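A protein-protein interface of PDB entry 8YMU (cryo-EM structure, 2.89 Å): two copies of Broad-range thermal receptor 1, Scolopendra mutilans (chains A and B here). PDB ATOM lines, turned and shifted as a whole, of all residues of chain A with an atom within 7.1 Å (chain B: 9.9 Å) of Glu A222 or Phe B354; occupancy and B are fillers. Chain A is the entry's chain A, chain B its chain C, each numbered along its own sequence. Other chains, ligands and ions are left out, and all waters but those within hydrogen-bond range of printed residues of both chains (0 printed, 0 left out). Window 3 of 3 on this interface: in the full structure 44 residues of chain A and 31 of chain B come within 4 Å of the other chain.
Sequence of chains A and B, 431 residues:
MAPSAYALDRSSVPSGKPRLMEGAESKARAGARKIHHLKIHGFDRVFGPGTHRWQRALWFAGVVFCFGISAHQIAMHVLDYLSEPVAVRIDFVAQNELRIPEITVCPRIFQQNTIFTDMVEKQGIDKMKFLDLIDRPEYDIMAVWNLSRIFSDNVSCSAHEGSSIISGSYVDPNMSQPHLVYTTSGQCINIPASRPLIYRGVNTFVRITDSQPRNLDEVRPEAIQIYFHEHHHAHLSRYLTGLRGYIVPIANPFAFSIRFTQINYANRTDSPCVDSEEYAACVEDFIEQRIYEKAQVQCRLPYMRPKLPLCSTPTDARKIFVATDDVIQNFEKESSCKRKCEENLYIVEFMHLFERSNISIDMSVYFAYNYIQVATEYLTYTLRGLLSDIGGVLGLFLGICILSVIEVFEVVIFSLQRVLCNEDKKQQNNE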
ATOM      1  N   ARG A 108      13.141  -9.738   0.013  1.00  0.00           N
ATOM      2  CA  ARG A 108      14.175  -8.883  -0.544  1.00  0.00           C
ATOM      3  C   ARG A 108      14.554  -9.388  -1.930  1.00  0.00           C
ATOM      4  O   ARG A 108      14.275 -10.534  -2.292  1.00  0.00           O
ATOM      5  CB  ARG A 108      15.393  -8.845   0.376  1.00  0.00           C
ATOM      6  CG  ARG A 108      15.262  -7.834   1.504  1.00  0.00           C
ATOM      7  CD  ARG A 108      16.590  -7.574   2.190  1.00  0.00           C
ATOM      8  NE  ARG A 108      17.134  -8.774   2.813  1.00  0.00           N
ATOM      9  CZ  ARG A 108      18.389  -8.904   3.218  1.00  0.00           C
ATOM     10  NH1 ARG A 108      19.271  -7.929   3.064  1.00  0.00           N
ATOM     11  NH2 ARG A 108      18.771 -10.040   3.792  1.00  0.00           N
ATOM     12  N   GLN A 112      19.298 -10.810  -2.619  1.00  0.00           N
ATOM     13  CA  GLN A 112      19.302 -10.564  -1.185  1.00  0.00           C
ATOM     14  C   GLN A 112      18.399 -11.521  -0.420  1.00  0.00           C
ATOM     15  O   GLN A 112      18.391 -11.487   0.814  1.00  0.00           O
ATOM     16  CB  GLN A 112      18.895  -9.117  -0.891  1.00  0.00           C
ATOM     17  CG  GLN A 112      19.987  -8.104  -1.180  1.00  0.00           C
ATOM     18  CD  GLN A 112      19.507  -6.675  -1.056  1.00  0.00           C
ATOM     19  OE1 GLN A 112      18.436  -6.412  -0.512  1.00  0.00           O
ATOM     20  NE2 GLN A 112      20.301  -5.739  -1.559  1.00  0.00           N
ATOM     21  N   THR A 114      17.666 -14.760   1.443  1.00  0.00           N
ATOM     22  CA  THR A 114      18.463 -15.758   2.134  1.00  0.00           C
ATOM     23  C   THR A 114      17.934 -17.170   1.921  1.00  0.00           C
ATOM     24  O   THR A 114      18.622 -18.134   2.270  1.00  0.00           O
ATOM     25  CB  THR A 114      18.512 -15.434   3.631  1.00  0.00           C
ATOM     26  OG1 THR A 114      19.100 -14.140   3.814  1.00  0.00           O
ATOM     27  CG2 THR A 114      19.343 -16.461   4.371  1.00  0.00           C
ATOM     28  N   ILE A 115      16.745 -17.316   1.342  1.00  0.00           N
ATOM     29  CA  ILE A 115      16.070 -18.548   0.960  1.00  0.00           C
ATOM     30  C   ILE A 115      16.282 -18.870  -0.512  1.00  0.00           C
ATOM     31  O   ILE A 115      16.692 -19.981  -0.853  1.00  0.00           O
ATOM     32  CB  ILE A 115      14.563 -18.470   1.289  1.00  0.00           C
ATOM     33  CG1 ILE A 115      14.354 -18.329   2.797  1.00  0.00           C
ATOM     34  CG2 ILE A 115      13.858 -19.703   0.756  1.00  0.00           C
ATOM     35  CD1 ILE A 115      12.930 -17.987   3.191  1.00  0.00           C
ATOM     36  N   ILE A 150       8.640 -16.674   0.550  1.00  0.00           N
ATOM     37  CA  ILE A 150       8.908 -16.651   1.982  1.00  0.00           C
ATOM     38  C   ILE A 150       7.621 -16.615   2.793  1.00  0.00           C
ATOM     39  O   ILE A 150       7.671 -16.505   4.023  1.00  0.00           O
ATOM     40  CB  ILE A 150       9.827 -15.476   2.364  1.00  0.00           C
ATOM     41  CG1 ILE A 150       9.127 -14.134   2.134  1.00  0.00           C
ATOM     42  CG2 ILE A 150      11.129 -15.545   1.586  1.00  0.00           C
ATOM     43  CD1 ILE A 150       9.779 -12.981   2.856  1.00  0.00           C
ATOM     44  N   ARG A 214       8.373 -22.557  12.262  1.00  0.00           N
ATOM     45  CA  ARG A 214       9.827 -22.434  12.165  1.00  0.00           C
ATOM     46  C   ARG A 214      10.464 -23.700  12.730  1.00  0.00           C
ATOM     47  O   ARG A 214      11.136 -23.697  13.765  1.00  0.00           O
ATOM     48  CB  ARG A 214      10.319 -21.187  12.889  1.00  0.00           C
ATOM     49  CG  ARG A 214      10.003 -19.886  12.168  1.00  0.00           C
ATOM     50  CD  ARG A 214      10.624 -18.695  12.878  1.00  0.00           C
ATOM     51  NE  ARG A 214      12.082 -18.750  12.860  1.00  0.00           N
ATOM     52  CZ  ARG A 214      12.846 -18.272  11.886  1.00  0.00           C
ATOM     53  NH1 ARG A 214      12.325 -17.696  10.814  1.00  0.00           N
ATOM     54  NH2 ARG A 214      14.168 -18.377  11.988  1.00  0.00           N
ATOM     55  N   ARG A 220      15.980 -19.285   7.085  1.00  0.00           N
ATOM     56  CA  ARG A 220      14.692 -18.626   6.943  1.00  0.00           C
ATOM     57  C   ARG A 220      14.861 -17.112   6.966  1.00  0.00           C
ATOM     58  O   ARG A 220      15.867 -16.589   7.456  1.00  0.00           O
ATOM     59  CB  ARG A 220      13.751 -19.104   8.051  1.00  0.00           C
ATOM     60  CG  ARG A 220      13.292 -20.535   7.825  1.00  0.00           C
ATOM     61  CD  ARG A 220      12.143 -20.946   8.722  1.00  0.00           C
ATOM     62  NE  ARG A 220      11.773 -22.336   8.481  1.00  0.00           N
ATOM     63  CZ  ARG A 220      11.067 -22.749   7.436  1.00  0.00           C
ATOM     64  NH1 ARG A 220      10.653 -21.905   6.504  1.00  0.00           N
ATOM     65  NH2 ARG A 220      10.781 -24.042   7.317  1.00  0.00           N
ATOM     66  N   PRO A 221      13.889 -16.366   6.443  1.00  0.00           N
ATOM     67  CA  PRO A 221      14.147 -14.977   6.056  1.00  0.00           C
ATOM     68  C   PRO A 221      14.325 -14.047   7.247  1.00  0.00           C
ATOM     69  O   PRO A 221      14.014 -14.377   8.392  1.00  0.00           O
ATOM     70  CB  PRO A 221      12.897 -14.611   5.255  1.00  0.00           C
ATOM     71  CG  PRO A 221      11.818 -15.384   5.915  1.00  0.00           C
ATOM     72  CD  PRO A 221      12.443 -16.659   6.437  1.00  0.00           C
ATOM     73  N   GLU A 222      14.844 -12.856   6.942  1.00  0.00           N
ATOM     74  CA  GLU A 222      15.175 -11.863   7.950  1.00  0.00           C
ATOM     75  C   GLU A 222      14.714 -10.452   7.612  1.00  0.00           C
ATOM     76  O   GLU A 222      14.847  -9.564   8.461  1.00  0.00           O
ATOM     77  CB  GLU A 222      16.693 -11.844   8.188  1.00  0.00           C
ATOM     78  CG  GLU A 222      17.502 -11.384   6.990  1.00  0.00           C
ATOM     79  CD  GLU A 222      18.992 -11.444   7.244  1.00  0.00           C
ATOM     80  OE1 GLU A 222      19.388 -11.867   8.350  1.00  0.00           O
ATOM     81  OE2 GLU A 222      19.768 -11.074   6.338  1.00  0.00           O
ATOM     82  N   ALA A 223      14.187 -10.213   6.414  1.00  0.00           N
ATOM     83  CA  ALA A 223      13.723  -8.886   6.038  1.00  0.00           C
ATOM     84  C   ALA A 223      12.651  -9.011   4.968  1.00  0.00           C
ATOM     85  O   ALA A 223      12.590 -10.007   4.244  1.00  0.00           O
ATOM     86  CB  ALA A 223      14.872  -8.013   5.528  1.00  0.00           C
ATOM     87  N   ILE A 224      11.809  -7.984   4.872  1.00  0.00           N
ATOM     88  CA  ILE A 224      10.739  -7.939   3.884  1.00  0.00           C
ATOM     89  C   ILE A 224      10.587  -6.514   3.370  1.00  0.00           C
ATOM     90  O   ILE A 224      10.822  -5.545   4.101  1.00  0.00           O
ATOM     91  CB  ILE A 224       9.402  -8.450   4.459  1.00  0.00           C
ATOM     92  CG1 ILE A 224       8.988  -7.625   5.677  1.00  0.00           C
ATOM     93  CG2 ILE A 224       9.511  -9.920   4.825  1.00  0.00           C
ATOM     94  CD1 ILE A 224       7.618  -7.966   6.186  1.00  0.00           C
ATOM     95  N   TYR A 246       9.743  -0.224   1.896  1.00  0.00           N
ATOM     96  CA  TYR A 246      10.550  -0.173   3.105  1.00  0.00           C
ATOM     97  C   TYR A 246      11.080  -1.568   3.408  1.00  0.00           C
ATOM     98  O   TYR A 246      10.305  -2.524   3.479  1.00  0.00           O
ATOM     99  CB  TYR A 246       9.716   0.328   4.284  1.00  0.00           C
ATOM    100  CG  TYR A 246       9.153   1.714   4.104  1.00  0.00           C
ATOM    101  CD1 TYR A 246       9.864   2.831   4.509  1.00  0.00           C
ATOM    102  CD2 TYR A 246       7.906   1.905   3.527  1.00  0.00           C
ATOM    103  CE1 TYR A 246       9.350   4.099   4.346  1.00  0.00           C
ATOM    104  CE2 TYR A 246       7.385   3.168   3.358  1.00  0.00           C
ATOM    105  CZ  TYR A 246       8.112   4.262   3.770  1.00  0.00           C
ATOM    106  OH  TYR A 246       7.597   5.526   3.604  1.00  0.00           O
ATOM    107  N   ILE A 247      12.389  -1.683   3.587  1.00  0.00           N
ATOM    108  CA  ILE A 247      13.019  -2.953   3.929  1.00  0.00           C
ATOM    109  C   ILE A 247      13.072  -3.032   5.448  1.00  0.00           C
ATOM    110  O   ILE A 247      13.877  -2.347   6.086  1.00  0.00           O
ATOM    111  CB  ILE A 247      14.415  -3.082   3.306  1.00  0.00           C
ATOM    112  CG1 ILE A 247      14.327  -2.946   1.785  1.00  0.00           C
ATOM    113  CG2 ILE A 247      15.033  -4.420   3.673  1.00  0.00           C
ATOM    114  CD1 ILE A 247      15.661  -2.814   1.100  1.00  0.00           C
ATOM    115  N   VAL A 248      12.217  -3.868   6.030  1.00  0.00           N
ATOM    116  CA  VAL A 248      12.071  -3.934   7.483  1.00  0.00           C
ATOM    117  C   VAL A 248      12.310  -5.359   7.967  1.00  0.00           C
ATOM    118  O   VAL A 248      11.997  -6.318   7.247  1.00  0.00           O
ATOM    119  CB  VAL A 248      10.684  -3.445   7.924  1.00  0.00           C
ATOM    120  CG1 VAL A 248      10.529  -1.966   7.636  1.00  0.00           C
ATOM    121  CG2 VAL A 248       9.587  -4.247   7.243  1.00  0.00           C
ATOM    122  N   PRO A 249      12.849  -5.547   9.169  1.00  0.00           N
ATOM    123  CA  PRO A 249      13.001  -6.904   9.704  1.00  0.00           C
ATOM    124  C   PRO A 249      11.760  -7.624  10.213  1.00  0.00           C
ATOM    125  O   PRO A 249      10.809  -7.003  10.693  1.00  0.00           O
ATOM    126  CB  PRO A 249      14.110  -6.761  10.753  1.00  0.00           C
ATOM    127  CG  PRO A 249      13.999  -5.336  11.222  1.00  0.00           C
ATOM    128  CD  PRO A 249      13.359  -4.529  10.107  1.00  0.00           C
ATOM    129  N   ILE A 250      11.784  -8.949  10.108  1.00  0.00           N
ATOM    130  CA  ILE A 250      10.682  -9.777  10.582  1.00  0.00           C
ATOM    131  C   ILE A 250      11.170 -10.677  11.707  1.00  0.00           C
ATOM    132  O   ILE A 250      10.543 -11.697  12.018  1.00  0.00           O
ATOM    133  CB  ILE A 250      10.077 -10.595   9.428  1.00  0.00           C
ATOM    134  CG1 ILE A 250      11.145 -11.474   8.778  1.00  0.00           C
ATOM    135  CG2 ILE A 250       9.462  -9.666   8.405  1.00  0.00           C
ATOM    136  CD1 ILE A 250      10.600 -12.460   7.779  1.00  0.00           C
ATOM    137  N   ALA A 251      12.291 -10.307  12.327  1.00  0.00           N
ATOM    138  CA  ALA A 251      12.781 -11.060  13.476  1.00  0.00           C
ATOM    139  C   ALA A 251      11.775 -11.017  14.618  1.00  0.00           C
ATOM    140  O   ALA A 251      11.502 -12.038  15.258  1.00  0.00           O
ATOM    141  CB  ALA A 251      14.134 -10.510  13.926  1.00  0.00           C
ATOM    142  N   PHE A 350       7.258   4.468  12.166  1.00  0.00           N
ATOM    143  CA  PHE A 350       7.406   3.183  12.832  1.00  0.00           C
ATOM    144  C   PHE A 350       6.925   3.305  14.271  1.00  0.00           C
ATOM    145  O   PHE A 350       7.229   4.288  14.954  1.00  0.00           O
ATOM    146  CB  PHE A 350       8.855   2.708  12.770  1.00  0.00           C
ATOM    147  CG  PHE A 350       9.296   2.330  11.387  1.00  0.00           C
ATOM    148  CD1 PHE A 350       9.549   3.304  10.437  1.00  0.00           C
ATOM    149  CD2 PHE A 350       9.436   1.001  11.028  1.00  0.00           C
ATOM    150  CE1 PHE A 350       9.946   2.963   9.164  1.00  0.00           C
ATOM    151  CE2 PHE A 350       9.834   0.656   9.757  1.00  0.00           C
ATOM    152  CZ  PHE A 350      10.089   1.638   8.823  1.00  0.00           C
ATOM    153  N   SER B 169      21.063  -1.875  -3.589  1.00  0.00           N
ATOM    154  CA  SER B 169      21.125  -0.441  -3.370  1.00  0.00           C
ATOM    155  C   SER B 169      22.276   0.171  -4.157  1.00  0.00           C
ATOM    156  O   SER B 169      23.327  -0.446  -4.347  1.00  0.00           O
ATOM    157  CB  SER B 169      21.285  -0.130  -1.883  1.00  0.00           C
ATOM    158  OG  SER B 169      21.282   1.268  -1.655  1.00  0.00           O
ATOM    159  N   ASN B 203      13.935   4.432  -0.367  1.00  0.00           N
ATOM    160  CA  ASN B 203      15.275   3.954  -0.036  1.00  0.00           C
ATOM    161  C   ASN B 203      16.329   4.906  -0.596  1.00  0.00           C
ATOM    162  O   ASN B 203      17.257   4.522  -1.307  1.00  0.00           O
ATOM    163  CB  ASN B 203      15.469   2.534  -0.559  1.00  0.00           C
ATOM    164  CG  ASN B 203      14.570   1.533   0.137  1.00  0.00           C
ATOM    165  OD1 ASN B 203      14.793   1.183   1.295  1.00  0.00           O
ATOM    166  ND2 ASN B 203      13.542   1.073  -0.565  1.00  0.00           N
ATOM    167  N   PHE B 205      18.839   7.386   1.121  1.00  0.00           N
ATOM    168  CA  PHE B 205      19.370   7.731   2.429  1.00  0.00           C
ATOM    169  C   PHE B 205      20.871   7.963   2.327  1.00  0.00           C
ATOM    170  O   PHE B 205      21.482   7.815   1.266  1.00  0.00           O
ATOM    171  CB  PHE B 205      19.046   6.641   3.455  1.00  0.00           C
ATOM    172  CG  PHE B 205      19.671   5.311   3.155  1.00  0.00           C
ATOM    173  CD1 PHE B 205      19.066   4.426   2.283  1.00  0.00           C
ATOM    174  CD2 PHE B 205      20.852   4.934   3.768  1.00  0.00           C
ATOM    175  CE1 PHE B 205      19.633   3.199   2.015  1.00  0.00           C
ATOM    176  CE2 PHE B 205      21.423   3.710   3.504  1.00  0.00           C
ATOM    177  CZ  PHE B 205      20.812   2.841   2.628  1.00  0.00           C
ATOM    178  N   ARG B 207      24.361   6.900   4.604  1.00  0.00           N
ATOM    179  CA  ARG B 207      24.892   6.059   5.666  1.00  0.00           C
ATOM    180  C   ARG B 207      26.235   6.599   6.133  1.00  0.00           C
ATOM    181  O   ARG B 207      27.162   6.748   5.334  1.00  0.00           O
ATOM    182  CB  ARG B 207      25.052   4.618   5.188  1.00  0.00           C
ATOM    183  CG  ARG B 207      25.034   3.598   6.310  1.00  0.00           C
ATOM    184  CD  ARG B 207      25.245   2.194   5.784  1.00  0.00           C
ATOM    185  NE  ARG B 207      25.961   1.362   6.744  1.00  0.00           N
ATOM    186  CZ  ARG B 207      26.816   0.400   6.423  1.00  0.00           C
ATOM    187  NH1 ARG B 207      27.094   0.110   5.162  1.00  0.00           N
ATOM    188  NH2 ARG B 207      27.409  -0.291   7.392  1.00  0.00           N
ATOM    189  N   PRO B 253      22.864  -0.308  15.027  1.00  0.00           N
ATOM    190  CA  PRO B 253      22.572   0.687  13.989  1.00  0.00           C
ATOM    191  C   PRO B 253      21.163   1.246  14.114  1.00  0.00           C
ATOM    192  O   PRO B 253      20.223   0.551  14.505  1.00  0.00           O
ATOM    193  CB  PRO B 253      22.761  -0.091  12.683  1.00  0.00           C
ATOM    194  CG  PRO B 253      23.574  -1.268  13.040  1.00  0.00           C
ATOM    195  CD  PRO B 253      23.262  -1.604  14.454  1.00  0.00           C
ATOM    196  N   PHE B 254      21.031   2.523  13.777  1.00  0.00           N
ATOM    197  CA  PHE B 254      19.791   3.271  13.882  1.00  0.00           C
ATOM    198  C   PHE B 254      19.557   4.023  12.580  1.00  0.00           C
ATOM    199  O   PHE B 254      20.471   4.217  11.776  1.00  0.00           O
ATOM    200  CB  PHE B 254      19.844   4.245  15.064  1.00  0.00           C
ATOM    201  CG  PHE B 254      21.041   5.148  15.040  1.00  0.00           C
ATOM    202  CD1 PHE B 254      22.291   4.673  15.397  1.00  0.00           C
ATOM    203  CD2 PHE B 254      20.917   6.469  14.658  1.00  0.00           C
ATOM    204  CE1 PHE B 254      23.391   5.497  15.367  1.00  0.00           C
ATOM    205  CE2 PHE B 254      22.014   7.295  14.634  1.00  0.00           C
ATOM    206  CZ  PHE B 254      23.251   6.808  14.985  1.00  0.00           C
ATOM    207  N   ALA B 255      18.314   4.446  12.371  1.00  0.00           N
ATOM    208  CA  ALA B 255      17.947   5.133  11.143  1.00  0.00           C
ATOM    209  C   ALA B 255      17.070   6.330  11.470  1.00  0.00           C
ATOM    210  O   ALA B 255      16.198   6.250  12.338  1.00  0.00           O
ATOM    211  CB  ALA B 255      17.218   4.193  10.178  1.00  0.00           C
ATOM    212  N   MET B 351      13.363   5.287  12.212  1.00  0.00           N
ATOM    213  CA  MET B 351      12.924   4.176  11.372  1.00  0.00           C
ATOM    214  C   MET B 351      13.515   2.894  11.934  1.00  0.00           C
ATOM    215  O   MET B 351      14.733   2.802  12.114  1.00  0.00           O
ATOM    216  CB  MET B 351      13.369   4.369   9.927  1.00  0.00           C
ATOM    217  CG  MET B 351      13.077   5.725   9.337  1.00  0.00           C
ATOM    218  SD  MET B 351      13.321   5.708   7.553  1.00  0.00           S
ATOM    219  CE  MET B 351      11.855   4.844   7.010  1.00  0.00           C
ATOM    220  N   HIS B 352      12.664   1.909  12.209  1.00  0.00           N
ATOM    221  CA  HIS B 352      13.156   0.580  12.540  1.00  0.00           C
ATOM    222  C   HIS B 352      13.265  -0.238  11.261  1.00  0.00           C
ATOM    223  O   HIS B 352      12.409  -1.082  10.984  1.00  0.00           O
ATOM    224  CB  HIS B 352      12.240  -0.113  13.548  1.00  0.00           C
ATOM    225  CG  HIS B 352      12.767  -1.430  14.027  1.00  0.00           C
ATOM    226  ND1 HIS B 352      14.065  -1.596  14.460  1.00  0.00           N
ATOM    227  CD2 HIS B 352      12.177  -2.643  14.136  1.00  0.00           C
ATOM    228  CE1 HIS B 352      14.251  -2.853  14.819  1.00  0.00           C
ATOM    229  NE2 HIS B 352      13.120  -3.510  14.631  1.00  0.00           N
ATOM    230  N   LEU B 353      14.306   0.013  10.474  1.00  0.00           N
ATOM    231  CA  LEU B 353      14.521  -0.644   9.195  1.00  0.00           C
ATOM    232  C   LEU B 353      15.519  -1.783   9.367  1.00  0.00           C
ATOM    233  O   LEU B 353      16.043  -2.024  10.458  1.00  0.00           O
ATOM    234  CB  LEU B 353      14.999   0.365   8.149  1.00  0.00           C
ATOM    235  CG  LEU B 353      13.945   1.354   7.649  1.00  0.00           C
ATOM    236  CD1 LEU B 353      14.475   2.165   6.491  1.00  0.00           C
ATOM    237  CD2 LEU B 353      12.685   0.621   7.240  1.00  0.00           C
ATOM    238  N   PHE B 354      15.780  -2.494   8.274  1.00  0.00           N
ATOM    239  CA  PHE B 354      16.654  -3.662   8.307  1.00  0.00           C
ATOM    240  C   PHE B 354      18.052  -3.421   7.751  1.00  0.00           C
ATOM    241  O   PHE B 354      18.248  -3.418   6.531  1.00  0.00           O
ATOM    242  CB  PHE B 354      16.024  -4.931   7.730  1.00  0.00           C
ATOM    243  CG  PHE B 354      17.000  -6.061   7.575  1.00  0.00           C
ATOM    244  CD1 PHE B 354      17.289  -6.894   8.640  1.00  0.00           C
ATOM    245  CD2 PHE B 354      17.651  -6.273   6.374  1.00  0.00           C
ATOM    246  CE1 PHE B 354      18.191  -7.927   8.505  1.00  0.00           C
ATOM    247  CE2 PHE B 354      18.556  -7.303   6.233  1.00  0.00           C
ATOM    248  CZ  PHE B 354      18.826  -8.130   7.300  1.00  0.00           C
ATOM    249  N   GLU B 355      19.011  -3.207   8.645  1.00  0.00           N
ATOM    250  CA  GLU B 355      20.419  -3.347   8.301  1.00  0.00           C
ATOM    251  C   GLU B 355      21.236  -3.397   9.583  1.00  0.00           C
ATOM    252  O   GLU B 355      21.164  -2.473  10.398  1.00  0.00           O
ATOM    253  CB  GLU B 355      20.884  -2.203   7.397  1.00  0.00           C
ATOM    254  CG  GLU B 355      20.975  -0.848   8.085  1.00  0.00           C
ATOM    255  CD  GLU B 355      22.377  -0.524   8.571  1.00  0.00           C
ATOM    256  OE1 GLU B 355      23.348  -1.117   8.055  1.00  0.00           O
ATOM    257  OE2 GLU B 355      22.508   0.329   9.474  1.00  0.00           O
ATOM    258  N   ARG B 356      21.993  -4.467   9.791  1.00  0.00           N
ATOM    259  CA  ARG B 356      22.915  -4.515  10.913  1.00  0.00           C
ATOM    260  C   ARG B 356      24.309  -4.907  10.442  1.00  0.00           C
ATOM    261  O   ARG B 356      24.485  -5.753   9.562  1.00  0.00           O
ATOM    262  CB  ARG B 356      22.439  -5.483  11.998  1.00  0.00           C
ATOM    263  CG  ARG B 356      22.915  -5.063  13.386  1.00  0.00           C
ATOM    264  CD  ARG B 356      23.026  -6.219  14.363  1.00  0.00           C
ATOM    265  NE  ARG B 356      23.431  -5.753  15.685  1.00  0.00           N
ATOM    266  CZ  ARG B 356      24.677  -5.454  16.030  1.00  0.00           C
ATOM    267  NH1 ARG B 356      25.679  -5.563  15.171  1.00  0.00           N
ATOM    268  NH2 ARG B 356      24.924  -5.029  17.265  1.00  0.00           N
ATOM    269  N   SER B 357      25.304  -4.268  11.050  1.00  0.00           N
ATOM    270  CA  SER B 357      26.707  -4.500  10.751  1.00  0.00           C
ATOM    271  C   SER B 357      27.448  -4.770  12.055  1.00  0.00           C
ATOM    272  O   SER B 357      26.844  -4.897  13.124  1.00  0.00           O
ATOM    273  CB  SER B 357      27.319  -3.306  10.009  1.00  0.00           C
ATOM    274  OG  SER B 357      28.503  -3.679   9.328  1.00  0.00           O
ATOM    275  N   ASP B 362      26.888   3.080  13.130  1.00  0.00           N
ATOM    276  CA  ASP B 362      26.262   2.833  11.835  1.00  0.00           C
ATOM    277  C   ASP B 362      24.976   3.649  11.814  1.00  0.00           C
ATOM    278  O   ASP B 362      23.941   3.212  12.324  1.00  0.00           O
ATOM    279  CB  ASP B 362      25.997   1.347  11.617  1.00  0.00           C
ATOM    280  CG  ASP B 362      25.481   1.042  10.224  1.00  0.00           C
ATOM    281  OD1 ASP B 362      25.026   1.975   9.531  1.00  0.00           O
ATOM    282  OD2 ASP B 362      25.535  -0.137   9.816  1.00  0.00           O
ATOM    283  N   SER B 364      22.038   5.865   9.704  1.00  0.00           N
ATOM    284  CA  SER B 364      21.345   6.054   8.442  1.00  0.00           C
ATOM    285  C   SER B 364      20.348   7.193   8.578  1.00  0.00           C
ATOM    286  O   SER B 364      19.554   7.234   9.521  1.00  0.00           O
ATOM    287  CB  SER B 364      20.623   4.778   8.004  1.00  0.00           C
ATOM    288  OG  SER B 364      21.542   3.723   7.784  1.00  0.00           O
ATOM    289  N   TYR B 366      17.401   8.746   6.366  1.00  0.00           N
ATOM    290  CA  TYR B 366      16.577   8.484   5.201  1.00  0.00           C
ATOM    291  C   TYR B 366      15.862   9.751   4.758  1.00  0.00           C
ATOM    292  O   TYR B 366      15.465  10.585   5.574  1.00  0.00           O
ATOM    293  CB  TYR B 366      15.551   7.389   5.497  1.00  0.00           C
ATOM    294  CG  TYR B 366      16.110   5.988   5.431  1.00  0.00           C
ATOM    295  CD1 TYR B 366      16.875   5.475   6.469  1.00  0.00           C
ATOM    296  CD2 TYR B 366      15.866   5.175   4.335  1.00  0.00           C
ATOM    297  CE1 TYR B 366      17.384   4.195   6.412  1.00  0.00           C
ATOM    298  CE2 TYR B 366      16.371   3.894   4.271  1.00  0.00           C
ATOM    299  CZ  TYR B 366      17.130   3.410   5.311  1.00  0.00           C
ATOM    300  OH  TYR B 366      17.633   2.132   5.250  1.00  0.00           O
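The backbone carbonyl oxygen (O) of Ile A247 lies within hydrogen-bond range of the backbone NH (N) of Phe B354 (2.9 Å).
Phe B354 touches Glu A222. CB of Ala A223 touches CD2 of Phe B354, 3.4 Å away. CE1 of Tyr A246 touches CE of Met B351 (3.7 Å). Ile A247 touches Leu B353. His B352 touches Val A248 (O to CG1, 3.9 Å). Val A248 touches Leu B353. His B352 touches Pro A249 (O to CD, 3.7 Å). Pro A249 touches Leu B353 (CD to C, 3.6 Å). Phe A350 touches Met B351. Phe A350 touches His B352 (CE2 to O, 3.3 Å).
No position is printed for both chains.
The guanidinium group (NH2) of Arg A108 sits at hydrogen-bond distance from the backbone carbonyl oxygen (O) of Gln A112. The guanidinium group of Arg A108 is in salt-bridge range of the side-chain carboxylate of Glu A222 (2.9 Å). The backbone NH (N) of Ile A224 is in hydrogen-bond range of the backbone carbonyl oxygen (O) of Val A248 (2.9 Å). N of Met B351 lies within hydrogen-bond range of O of Ala B255 (3.0 Å).
Hydrophobic or aromatic side chains of chain A within 4 Å of the printed part of chain B: Ala A223, Tyr A246, Val A248, Pro A249 and Phe A350. Along chain A the printed residues that touch a printed residue of chain B span positions 108 to 350. Among the printed residues, 15 pairs touch across the chains. Among the printed residues, no Asp or Glu carboxylate lies within 4 Å of a Lys or Arg side-chain nitrogen of the other chain.
Printed residues of chain B within 4 Å of Glu A222: Phe B354. Of chain A, only Arg A108, Glu A222, Ala A223, Ile A247, Val A248 and Pro A249 come within 4 Å of Phe B354. No residue of chain B comes within 4 Å of Pro A221. Of chain B, only Phe B354 (3.4 Å) comes within 4 Å of Ala A223. Of the printed residues of chain A, Met B351 touches Tyr A246 and Phe A350. Printed residues of chain A within 4 Å of His B352: Val A248 (3.9 Å), Pro A249 (3.7 Å) and Phe A350 (3.3 Å). Ile A250 touches none of the printed residues of chain B. The nearest residue of chain B that does not touch Glu A222 is Glu B355 (7.6 Å). The nearest printed residue of chain A that does not touch Leu B353 is Tyr A246 (4.2 Å).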
